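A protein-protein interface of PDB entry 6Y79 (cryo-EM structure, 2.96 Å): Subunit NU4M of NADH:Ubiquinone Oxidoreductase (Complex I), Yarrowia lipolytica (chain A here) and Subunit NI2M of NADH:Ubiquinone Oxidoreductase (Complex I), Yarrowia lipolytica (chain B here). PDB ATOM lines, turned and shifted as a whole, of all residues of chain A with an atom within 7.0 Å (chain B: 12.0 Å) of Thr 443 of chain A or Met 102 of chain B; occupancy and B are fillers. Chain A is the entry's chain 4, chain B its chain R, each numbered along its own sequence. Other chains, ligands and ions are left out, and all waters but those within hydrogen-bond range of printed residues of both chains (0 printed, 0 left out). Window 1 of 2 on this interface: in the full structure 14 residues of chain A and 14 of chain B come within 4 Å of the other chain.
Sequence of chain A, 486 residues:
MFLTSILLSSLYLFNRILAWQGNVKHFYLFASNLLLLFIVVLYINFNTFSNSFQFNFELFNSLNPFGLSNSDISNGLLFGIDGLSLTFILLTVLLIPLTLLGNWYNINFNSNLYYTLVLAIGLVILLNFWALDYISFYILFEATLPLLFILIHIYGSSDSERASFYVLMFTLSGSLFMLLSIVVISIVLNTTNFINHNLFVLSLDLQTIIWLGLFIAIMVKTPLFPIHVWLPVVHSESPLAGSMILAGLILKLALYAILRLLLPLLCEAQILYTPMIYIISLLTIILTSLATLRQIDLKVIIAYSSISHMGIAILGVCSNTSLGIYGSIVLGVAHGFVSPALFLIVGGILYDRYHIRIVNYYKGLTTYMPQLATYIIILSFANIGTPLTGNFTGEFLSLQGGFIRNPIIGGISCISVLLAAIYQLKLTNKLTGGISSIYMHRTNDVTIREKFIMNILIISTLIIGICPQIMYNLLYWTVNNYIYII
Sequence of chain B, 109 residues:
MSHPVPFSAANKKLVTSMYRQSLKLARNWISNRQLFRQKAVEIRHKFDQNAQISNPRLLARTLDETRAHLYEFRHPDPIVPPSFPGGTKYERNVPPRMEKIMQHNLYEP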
ATOM      1  N   ILE A 349     -21.181  -9.698 -18.445  1.00  0.00           N
ATOM      2  CA  ILE A 349     -21.835  -8.482 -17.981  1.00  0.00           C
ATOM      3  C   ILE A 349     -23.268  -8.752 -17.532  1.00  0.00           C
ATOM      4  O   ILE A 349     -23.881  -7.925 -16.853  1.00  0.00           O
ATOM      5  CB  ILE A 349     -21.743  -7.439 -19.107  1.00  0.00           C
ATOM      6  CG1 ILE A 349     -20.330  -7.443 -19.689  1.00  0.00           C
ATOM      7  CG2 ILE A 349     -22.066  -6.063 -18.610  1.00  0.00           C
ATOM      8  CD1 ILE A 349     -20.078  -6.380 -20.720  1.00  0.00           C
ATOM      9  N   ARG A 353     -24.013 -10.098 -12.854  1.00  0.00           N
ATOM     10  CA  ARG A 353     -24.830  -9.104 -12.181  1.00  0.00           C
ATOM     11  C   ARG A 353     -26.135  -9.681 -11.655  1.00  0.00           C
ATOM     12  O   ARG A 353     -26.585  -9.278 -10.581  1.00  0.00           O
ATOM     13  CB  ARG A 353     -25.139  -7.935 -13.124  1.00  0.00           C
ATOM     14  CG  ARG A 353     -24.128  -6.787 -13.172  1.00  0.00           C
ATOM     15  CD  ARG A 353     -22.869  -7.187 -13.907  1.00  0.00           C
ATOM     16  NE  ARG A 353     -22.033  -6.083 -14.357  1.00  0.00           N
ATOM     17  CZ  ARG A 353     -20.790  -6.248 -14.798  1.00  0.00           C
ATOM     18  NH1 ARG A 353     -20.074  -5.209 -15.191  1.00  0.00           N
ATOM     19  NH2 ARG A 353     -20.257  -7.464 -14.845  1.00  0.00           N
ATOM     20  N   TYR A 354     -26.752 -10.628 -12.365  1.00  0.00           N
ATOM     21  CA  TYR A 354     -28.083 -11.093 -12.004  1.00  0.00           C
ATOM     22  C   TYR A 354     -28.212 -12.593 -11.809  1.00  0.00           C
ATOM     23  O   TYR A 354     -29.222 -13.024 -11.249  1.00  0.00           O
ATOM     24  CB  TYR A 354     -29.105 -10.641 -13.056  1.00  0.00           C
ATOM     25  CG  TYR A 354     -29.138  -9.145 -13.172  1.00  0.00           C
ATOM     26  CD1 TYR A 354     -29.789  -8.379 -12.221  1.00  0.00           C
ATOM     27  CD2 TYR A 354     -28.489  -8.496 -14.205  1.00  0.00           C
ATOM     28  CE1 TYR A 354     -29.804  -7.013 -12.304  1.00  0.00           C
ATOM     29  CE2 TYR A 354     -28.496  -7.128 -14.293  1.00  0.00           C
ATOM     30  CZ  TYR A 354     -29.157  -6.394 -13.339  1.00  0.00           C
ATOM     31  OH  TYR A 354     -29.173  -5.028 -13.427  1.00  0.00           O
ATOM     32  N   TYR A 368     -30.583   2.347 -17.825  1.00  0.00           N
ATOM     33  CA  TYR A 368     -29.608   2.284 -16.753  1.00  0.00           C
ATOM     34  C   TYR A 368     -28.214   1.950 -17.242  1.00  0.00           C
ATOM     35  O   TYR A 368     -27.243   2.273 -16.556  1.00  0.00           O
ATOM     36  CB  TYR A 368     -30.009   1.235 -15.707  1.00  0.00           C
ATOM     37  CG  TYR A 368     -31.247   1.558 -14.910  1.00  0.00           C
ATOM     38  CD1 TYR A 368     -31.662   2.870 -14.718  1.00  0.00           C
ATOM     39  CD2 TYR A 368     -32.010   0.541 -14.355  1.00  0.00           C
ATOM     40  CE1 TYR A 368     -32.797   3.155 -13.995  1.00  0.00           C
ATOM     41  CE2 TYR A 368     -33.144   0.815 -13.634  1.00  0.00           C
ATOM     42  CZ  TYR A 368     -33.533   2.122 -13.457  1.00  0.00           C
ATOM     43  OH  TYR A 368     -34.665   2.392 -12.733  1.00  0.00           O
ATOM     44  N   MET A 369     -28.096   1.292 -18.392  1.00  0.00           N
ATOM     45  CA  MET A 369     -26.816   0.869 -18.953  1.00  0.00           C
ATOM     46  C   MET A 369     -26.774   1.290 -20.409  1.00  0.00           C
ATOM     47  O   MET A 369     -27.058   0.486 -21.303  1.00  0.00           O
ATOM     48  CB  MET A 369     -26.637  -0.640 -18.842  1.00  0.00           C
ATOM     49  CG  MET A 369     -26.605  -1.168 -17.444  1.00  0.00           C
ATOM     50  SD  MET A 369     -26.710  -2.947 -17.489  1.00  0.00           S
ATOM     51  CE  MET A 369     -26.270  -3.325 -15.818  1.00  0.00           C
ATOM     52  N   MET A 440     -35.224  -6.763 -12.554  1.00  0.00           N
ATOM     53  CA  MET A 440     -33.846  -6.332 -12.371  1.00  0.00           C
ATOM     54  C   MET A 440     -33.802  -5.085 -11.504  1.00  0.00           C
ATOM     55  O   MET A 440     -34.429  -4.073 -11.828  1.00  0.00           O
ATOM     56  CB  MET A 440     -33.184  -6.035 -13.712  1.00  0.00           C
ATOM     57  CG  MET A 440     -33.149  -7.167 -14.707  1.00  0.00           C
ATOM     58  SD  MET A 440     -32.960  -6.444 -16.344  1.00  0.00           S
ATOM     59  CE  MET A 440     -31.247  -5.932 -16.308  1.00  0.00           C
ATOM     60  N   HIS A 441     -33.058  -5.152 -10.411  1.00  0.00           N
ATOM     61  CA  HIS A 441     -32.638  -3.937  -9.743  1.00  0.00           C
ATOM     62  C   HIS A 441     -31.382  -3.408 -10.416  1.00  0.00           C
ATOM     63  O   HIS A 441     -30.596  -4.164 -10.988  1.00  0.00           O
ATOM     64  CB  HIS A 441     -32.387  -4.185  -8.259  1.00  0.00           C
ATOM     65  CG  HIS A 441     -32.205  -2.933  -7.465  1.00  0.00           C
ATOM     66  ND1 HIS A 441     -30.976  -2.334  -7.297  1.00  0.00           N
ATOM     67  CD2 HIS A 441     -33.095  -2.153  -6.810  1.00  0.00           C
ATOM     68  CE1 HIS A 441     -31.115  -1.245  -6.564  1.00  0.00           C
ATOM     69  NE2 HIS A 441     -32.391  -1.110  -6.258  1.00  0.00           N
ATOM     70  N   ARG A 442     -31.213  -2.095 -10.358  1.00  0.00           N
ATOM     71  CA  ARG A 442     -30.140  -1.417 -11.063  1.00  0.00           C
ATOM     72  C   ARG A 442     -28.773  -1.793 -10.510  1.00  0.00           C
ATOM     73  O   ARG A 442     -28.556  -1.772  -9.300  1.00  0.00           O
ATOM     74  CB  ARG A 442     -30.341   0.079 -10.929  1.00  0.00           C
ATOM     75  CG  ARG A 442     -29.238   0.878 -11.479  1.00  0.00           C
ATOM     76  CD  ARG A 442     -29.330   2.270 -11.022  1.00  0.00           C
ATOM     77  NE  ARG A 442     -28.644   3.090 -12.003  1.00  0.00           N
ATOM     78  CZ  ARG A 442     -28.771   4.403 -12.103  1.00  0.00           C
ATOM     79  NH1 ARG A 442     -29.552   5.060 -11.261  1.00  0.00           N
ATOM     80  NH2 ARG A 442     -28.127   5.042 -13.051  1.00  0.00           N
ATOM     81  N   THR A 443     -27.840  -2.122 -11.398  1.00  0.00           N
ATOM     82  CA  THR A 443     -26.475  -2.437 -11.005  1.00  0.00           C
ATOM     83  C   THR A 443     -25.496  -1.493 -11.694  1.00  0.00           C
ATOM     84  O   THR A 443     -25.885  -0.496 -12.304  1.00  0.00           O
ATOM     85  CB  THR A 443     -26.132  -3.892 -11.314  1.00  0.00           C
ATOM     86  OG1 THR A 443     -26.405  -4.162 -12.687  1.00  0.00           O
ATOM     87  CG2 THR A 443     -26.950  -4.816 -10.470  1.00  0.00           C
ATOM     88  N   ASN A 444     -24.213  -1.805 -11.554  1.00  0.00           N
ATOM     89  CA  ASN A 444     -23.150  -1.008 -12.138  1.00  0.00           C
ATOM     90  C   ASN A 444     -23.214  -1.052 -13.654  1.00  0.00           C
ATOM     91  O   ASN A 444     -23.671  -2.020 -14.258  1.00  0.00           O
ATOM     92  CB  ASN A 444     -21.784  -1.525 -11.697  1.00  0.00           C
ATOM     93  CG  ASN A 444     -21.537  -1.334 -10.231  1.00  0.00           C
ATOM     94  OD1 ASN A 444     -21.483  -0.212  -9.742  1.00  0.00           O
ATOM     95  ND2 ASN A 444     -21.381  -2.436  -9.511  1.00  0.00           N
ATOM     96  N   ASP A 445     -22.719   0.008 -14.276  1.00  0.00           N
ATOM     97  CA  ASP A 445     -22.489  -0.056 -15.705  1.00  0.00           C
ATOM     98  C   ASP A 445     -21.214  -0.845 -15.985  1.00  0.00           C
ATOM     99  O   ASP A 445     -20.523  -1.308 -15.072  1.00  0.00           O
ATOM    100  CB  ASP A 445     -22.401   1.342 -16.304  1.00  0.00           C
ATOM    101  CG  ASP A 445     -22.989   1.412 -17.696  1.00  0.00           C
ATOM    102  OD1 ASP A 445     -23.391   0.361 -18.230  1.00  0.00           O
ATOM    103  OD2 ASP A 445     -23.042   2.523 -18.260  1.00  0.00           O
ATOM    104  N   PRO B  96     -37.326   7.299 -15.423  1.00  0.00           N
ATOM    105  CA  PRO B  96     -36.767   6.152 -14.706  1.00  0.00           C
ATOM    106  C   PRO B  96     -36.965   6.307 -13.209  1.00  0.00           C
ATOM    107  O   PRO B  96     -36.922   7.416 -12.674  1.00  0.00           O
ATOM    108  CB  PRO B  96     -35.285   6.190 -15.082  1.00  0.00           C
ATOM    109  CG  PRO B  96     -35.029   7.603 -15.435  1.00  0.00           C
ATOM    110  CD  PRO B  96     -36.281   8.124 -16.047  1.00  0.00           C
ATOM    111  N   ARG B  97     -37.217   5.190 -12.539  1.00  0.00           N
ATOM    112  CA  ARG B  97     -37.413   5.244 -11.101  1.00  0.00           C
ATOM    113  C   ARG B  97     -36.078   5.494 -10.410  1.00  0.00           C
ATOM    114  O   ARG B  97     -35.018   5.113 -10.913  1.00  0.00           O
ATOM    115  CB  ARG B  97     -38.069   3.958 -10.602  1.00  0.00           C
ATOM    116  CG  ARG B  97     -37.201   2.730 -10.651  1.00  0.00           C
ATOM    117  CD  ARG B  97     -38.004   1.486 -10.348  1.00  0.00           C
ATOM    118  NE  ARG B  97     -39.010   1.230 -11.373  1.00  0.00           N
ATOM    119  CZ  ARG B  97     -38.777   0.570 -12.501  1.00  0.00           C
ATOM    120  NH1 ARG B  97     -37.569   0.099 -12.768  1.00  0.00           N
ATOM    121  NH2 ARG B  97     -39.757   0.381 -13.370  1.00  0.00           N
ATOM    122  N   MET B  98     -36.127   6.193  -9.282  1.00  0.00           N
ATOM    123  CA  MET B  98     -34.904   6.569  -8.583  1.00  0.00           C
ATOM    124  C   MET B  98     -34.348   5.358  -7.857  1.00  0.00           C
ATOM    125  O   MET B  98     -34.949   4.866  -6.898  1.00  0.00           O
ATOM    126  CB  MET B  98     -35.170   7.718  -7.618  1.00  0.00           C
ATOM    127  CG  MET B  98     -35.403   9.032  -8.326  1.00  0.00           C
ATOM    128  SD  MET B  98     -34.184   9.273  -9.627  1.00  0.00           S
ATOM    129  CE  MET B  98     -34.909  10.655 -10.480  1.00  0.00           C
ATOM    130  N   GLU B  99     -33.201   4.871  -8.315  1.00  0.00           N
ATOM    131  CA  GLU B  99     -32.599   3.662  -7.783  1.00  0.00           C
ATOM    132  C   GLU B  99     -31.112   3.882  -7.598  1.00  0.00           C
ATOM    133  O   GLU B  99     -30.433   4.344  -8.518  1.00  0.00           O
ATOM    134  CB  GLU B  99     -32.832   2.476  -8.711  1.00  0.00           C
ATOM    135  CG  GLU B  99     -34.187   1.838  -8.574  1.00  0.00           C
ATOM    136  CD  GLU B  99     -34.354   0.669  -9.511  1.00  0.00           C
ATOM    137  OE1 GLU B  99     -33.566   0.573 -10.470  1.00  0.00           O
ATOM    138  OE2 GLU B  99     -35.262  -0.157  -9.292  1.00  0.00           O
ATOM    139  N   LYS B 100     -30.612   3.558  -6.414  1.00  0.00           N
ATOM    140  CA  LYS B 100     -29.176   3.557  -6.228  1.00  0.00           C
ATOM    141  C   LYS B 100     -28.604   2.237  -6.731  1.00  0.00           C
ATOM    142  O   LYS B 100     -29.314   1.247  -6.903  1.00  0.00           O
ATOM    143  CB  LYS B 100     -28.813   3.792  -4.760  1.00  0.00           C
ATOM    144  CG  LYS B 100     -28.643   5.263  -4.371  1.00  0.00           C
ATOM    145  CD  LYS B 100     -29.982   5.960  -4.173  1.00  0.00           C
ATOM    146  CE  LYS B 100     -30.716   5.409  -2.964  1.00  0.00           C
ATOM    147  NZ  LYS B 100     -32.070   6.011  -2.817  1.00  0.00           N
ATOM    148  N   ILE B 101     -27.299   2.235  -6.968  1.00  0.00           N
ATOM    149  CA  ILE B 101     -26.650   1.131  -7.661  1.00  0.00           C
ATOM    150  C   ILE B 101     -26.451  -0.036  -6.703  1.00  0.00           C
ATOM    151  O   ILE B 101     -25.780   0.097  -5.676  1.00  0.00           O
ATOM    152  CB  ILE B 101     -25.314   1.579  -8.258  1.00  0.00           C
ATOM    153  CG1 ILE B 101     -25.540   2.635  -9.331  1.00  0.00           C
ATOM    154  CG2 ILE B 101     -24.586   0.411  -8.832  1.00  0.00           C
ATOM    155  CD1 ILE B 101     -24.271   3.270  -9.813  1.00  0.00           C
ATOM    156  N   MET B 102     -27.035  -1.182  -7.040  1.00  0.00           N
ATOM    157  CA  MET B 102     -26.737  -2.428  -6.352  1.00  0.00           C
ATOM    158  C   MET B 102     -25.413  -2.966  -6.866  1.00  0.00           C
ATOM    159  O   MET B 102     -25.102  -2.839  -8.050  1.00  0.00           O
ATOM    160  CB  MET B 102     -27.855  -3.439  -6.591  1.00  0.00           C
ATOM    161  CG  MET B 102     -27.720  -4.749  -5.866  1.00  0.00           C
ATOM    162  SD  MET B 102     -28.187  -4.576  -4.152  1.00  0.00           S
ATOM    163  CE  MET B 102     -29.910  -4.153  -4.347  1.00  0.00           C
ATOM    164  N   GLN B 103     -24.617  -3.552  -5.984  1.00  0.00           N
ATOM    165  CA  GLN B 103     -23.287  -3.983  -6.372  1.00  0.00           C
ATOM    166  C   GLN B 103     -23.143  -5.491  -6.246  1.00  0.00           C
ATOM    167  O   GLN B 103     -23.710  -6.119  -5.350  1.00  0.00           O
ATOM    168  CB  GLN B 103     -22.230  -3.249  -5.563  1.00  0.00           C
ATOM    169  CG  GLN B 103     -22.119  -1.818  -6.023  1.00  0.00           C
ATOM    170  CD  GLN B 103     -21.045  -1.054  -5.324  1.00  0.00           C
ATOM    171  OE1 GLN B 103     -20.339  -1.592  -4.471  1.00  0.00           O
ATOM    172  NE2 GLN B 103     -20.895   0.213  -5.682  1.00  0.00           N
ATOM    173  N   HIS B 104     -22.382  -6.061  -7.175  1.00  0.00           N
ATOM    174  CA  HIS B 104     -22.298  -7.496  -7.365  1.00  0.00           C
ATOM    175  C   HIS B 104     -20.897  -8.050  -7.167  1.00  0.00           C
ATOM    176  O   HIS B 104     -20.738  -9.272  -7.114  1.00  0.00           O
ATOM    177  CB  HIS B 104     -22.778  -7.866  -8.777  1.00  0.00           C
ATOM    178  CG  HIS B 104     -21.894  -7.327  -9.857  1.00  0.00           C
ATOM    179  ND1 HIS B 104     -21.943  -6.016 -10.270  1.00  0.00           N
ATOM    180  CD2 HIS B 104     -20.910  -7.912 -10.577  1.00  0.00           C
ATOM    181  CE1 HIS B 104     -21.035  -5.819 -11.208  1.00  0.00           C
ATOM    182  NE2 HIS B 104     -20.393  -6.953 -11.411  1.00  0.00           N
ATOM    183  N   ASN B 105     -19.886  -7.202  -7.048  1.00  0.00           N
ATOM    184  CA  ASN B 105     -18.509  -7.654  -6.967  1.00  0.00           C
ATOM    185  C   ASN B 105     -17.793  -6.920  -5.844  1.00  0.00           C
ATOM    186  O   ASN B 105     -18.024  -5.730  -5.620  1.00  0.00           O
ATOM    187  CB  ASN B 105     -17.795  -7.433  -8.302  1.00  0.00           C
ATOM    188  CG  ASN B 105     -16.490  -8.176  -8.393  1.00  0.00           C
ATOM    189  OD1 ASN B 105     -16.185  -9.034  -7.566  1.00  0.00           O
ATOM    190  ND2 ASN B 105     -15.714  -7.862  -9.413  1.00  0.00           N
ATOM    191  N   LEU B 106     -16.926  -7.645  -5.142  1.00  0.00           N
ATOM    192  CA  LEU B 106     -16.174  -7.058  -4.042  1.00  0.00           C
ATOM    193  C   LEU B 106     -15.093  -6.110  -4.535  1.00  0.00           C
ATOM    194  O   LEU B 106     -14.746  -5.149  -3.847  1.00  0.00           O
ATOM    195  CB  LEU B 106     -15.547  -8.173  -3.210  1.00  0.00           C
ATOM    196  CG  LEU B 106     -14.700  -7.854  -1.982  1.00  0.00           C
ATOM    197  CD1 LEU B 106     -15.544  -7.204  -0.935  1.00  0.00           C
ATOM    198  CD2 LEU B 106     -14.068  -9.114  -1.439  1.00  0.00           C
ATOM    199  N   TYR B 107     -14.551  -6.348  -5.720  1.00  0.00           N
ATOM    200  CA  TYR B 107     -13.323  -5.693  -6.139  1.00  0.00           C
ATOM    201  C   TYR B 107     -13.558  -4.598  -7.163  1.00  0.00           C
ATOM    202  O   TYR B 107     -12.890  -3.559  -7.144  1.00  0.00           O
ATOM    203  CB  TYR B 107     -12.363  -6.735  -6.706  1.00  0.00           C
ATOM    204  CG  TYR B 107     -12.019  -7.826  -5.726  1.00  0.00           C
ATOM    205  CD1 TYR B 107     -10.995  -7.657  -4.808  1.00  0.00           C
ATOM    206  CD2 TYR B 107     -12.720  -9.026  -5.712  1.00  0.00           C
ATOM    207  CE1 TYR B 107     -10.680  -8.644  -3.909  1.00  0.00           C
ATOM    208  CE2 TYR B 107     -12.410 -10.017  -4.812  1.00  0.00           C
ATOM    209  CZ  TYR B 107     -11.390  -9.822  -3.916  1.00  0.00           C
ATOM    210  OH  TYR B 107     -11.076 -10.815  -3.020  1.00  0.00           O
ATOM    211  N   GLU B 108     -14.511  -4.809  -8.050  1.00  0.00           N
ATOM    212  CA  GLU B 108     -14.723  -4.002  -9.235  1.00  0.00           C
ATOM    213  C   GLU B 108     -16.130  -3.426  -9.191  1.00  0.00           C
ATOM    214  O   GLU B 108     -17.037  -4.068  -8.661  1.00  0.00           O
ATOM    215  CB  GLU B 108     -14.542  -4.892 -10.466  1.00  0.00           C
ATOM    216  CG  GLU B 108     -15.061  -4.408 -11.791  1.00  0.00           C
ATOM    217  CD  GLU B 108     -15.353  -5.572 -12.723  1.00  0.00           C
ATOM    218  OE1 GLU B 108     -16.098  -6.486 -12.314  1.00  0.00           O
ATOM    219  OE2 GLU B 108     -14.820  -5.600 -13.847  1.00  0.00           O
ATOM    220  N   PRO B 109     -16.330  -2.191  -9.653  1.00  0.00           N
ATOM    221  CA  PRO B 109     -17.725  -1.769  -9.785  1.00  0.00           C
ATOM    222  C   PRO B 109     -18.426  -2.514 -10.906  1.00  0.00           C
ATOM    223  O   PRO B 109     -19.048  -3.525 -10.592  1.00  0.00           O
ATOM    224  CB  PRO B 109     -17.604  -0.285 -10.103  1.00  0.00           C
ATOM    225  CG  PRO B 109     -16.312   0.125  -9.529  1.00  0.00           C
ATOM    226  CD  PRO B 109     -15.407  -1.053  -9.749  1.00  0.00           C
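Among the printed residues, pairs that only touch across the chains: His 441 of chain A with Lys 100 of chain B (3.1 Å), Thr 443 of chain A with Met 102 of chain B (3.3 Å), Asn 444 of chain A with Ile 101 of chain B (3.3 Å), His 441 of chain A with Met 102 of chain B (3.4 Å), Thr 443 of chain A with Ile 101 of chain B (3.6 Å), Asn 444 of chain A with Gln 103 of chain B (3.6 Å), Asn 444 of chain A with His 104 of chain B (3.7 Å), Asn 444 of chain A with Met 102 of chain B (3.8 Å), Arg 442 of chain A with Ile 101 of chain B (3.8 Å), His 441 of chain A with Glu 99 of chain B (3.9 Å) and Arg 442 of chain A with Lys 100 of chain B (3.9 Å).
Of the 14 printed residues of chain B, 8 touch a printed residue of chain A.
Printed residues of chain B that touch a printed residue of chain A: Arg 97, Glu 99, Lys 100, Ile 101, Met 102, Gln 103, His 104 and Pro 109.
Hydrophobic or aromatic side chains of chain B within 4 Å of the printed part of chain A: Ile 101, Met 102, His 104 and Pro 109.
Of the 11 printed residues of chain A, 6 touch a printed residue of chain B.
Printed residues of chain A that touch a printed residue of chain B: Arg 353, Tyr 368, His 441, Arg 442, Thr 443 and Asn 444.
Hydrophobic or aromatic side chains of chain A that line the printed part of chain B: Tyr 368 and His 441.
Among the printed residues, 17 pairs touch across the chains.
The backbone carbonyl oxygen (O) of Arg 442 of chain A sits at hydrogen-bond distance from the backbone NH (N) of Met 102 of chain B, 2.8 Å away.
The side-chain hydroxyl (OH) of Tyr 368 of chain A is in hydrogen-bond range of the backbone carbonyl oxygen (O) of Arg 97 of chain B, 3.3 Å away.
The guanidinium group of Arg 442 of chain A lies within hydrogen-bond range of the backbone carbonyl oxygen of Glu 99 of chain B.
The side-chain amide nitrogen (ND2) of Asn 444 of chain A sits at hydrogen-bond distance from the backbone carbonyl oxygen (O) of Pro 109 of chain B (2.8 Å).
NE2 of His 104 of chain B sits at hydrogen-bond distance from NH2 of Arg 353 of chain A, 3.5 Å away.
The side-chain carboxylate (OE1) of Glu 99 of chain B is in hydrogen-bond range of the side-chain hydroxyl (OH) of Tyr 368 of chain A.
Thr 443 of chain A touches just these residues of chain B: Ile 101 (3.6 Å) and Met 102 (3.3 Å).
Of the printed residues of chain A, Met 102 of chain B touches His 441 (3.4 Å), Arg 442 (2.8 Å), Thr 443 (3.3 Å) and Asn 444 (3.8 Å).
Of the printed residues of chain B, His 441 of chain A touches Glu 99 (3.9 Å), Lys 100 (3.1 Å) and Met 102 (3.4 Å).
Arg 442 of chain A touches four residues of chain B.
Printed residues of chain B within 4 Å of Asn 444 of chain A: Ile 101 (3.3 Å), Met 102 (3.8 Å), Gln 103 (3.6 Å), His 104 (3.7 Å) and Pro 109 (2.8 Å).
Printed residues of chain B within 4 Å of Tyr 368 of chain A: Arg 97 (3.3 Å) and Glu 99 (3.1 Å).
Of the printed residues of chain A, His 104 of chain B touches Arg 353 (3.3 Å) and Asn 444 (3.7 Å).
Tyr 107 of chain B touches none of the printed residues of chain A.
The nearest residue of chain A that does not touch Met 102 of chain B is Arg 353 of chain A (6.5 Å).
O of His 441 of chain A lies within hydrogen-bond range of OH of Tyr 354 of chain A (3.0 Å).
OH of Tyr 354 of chain A lies within hydrogen-bond range of OG1 of Thr 443 of chain A.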
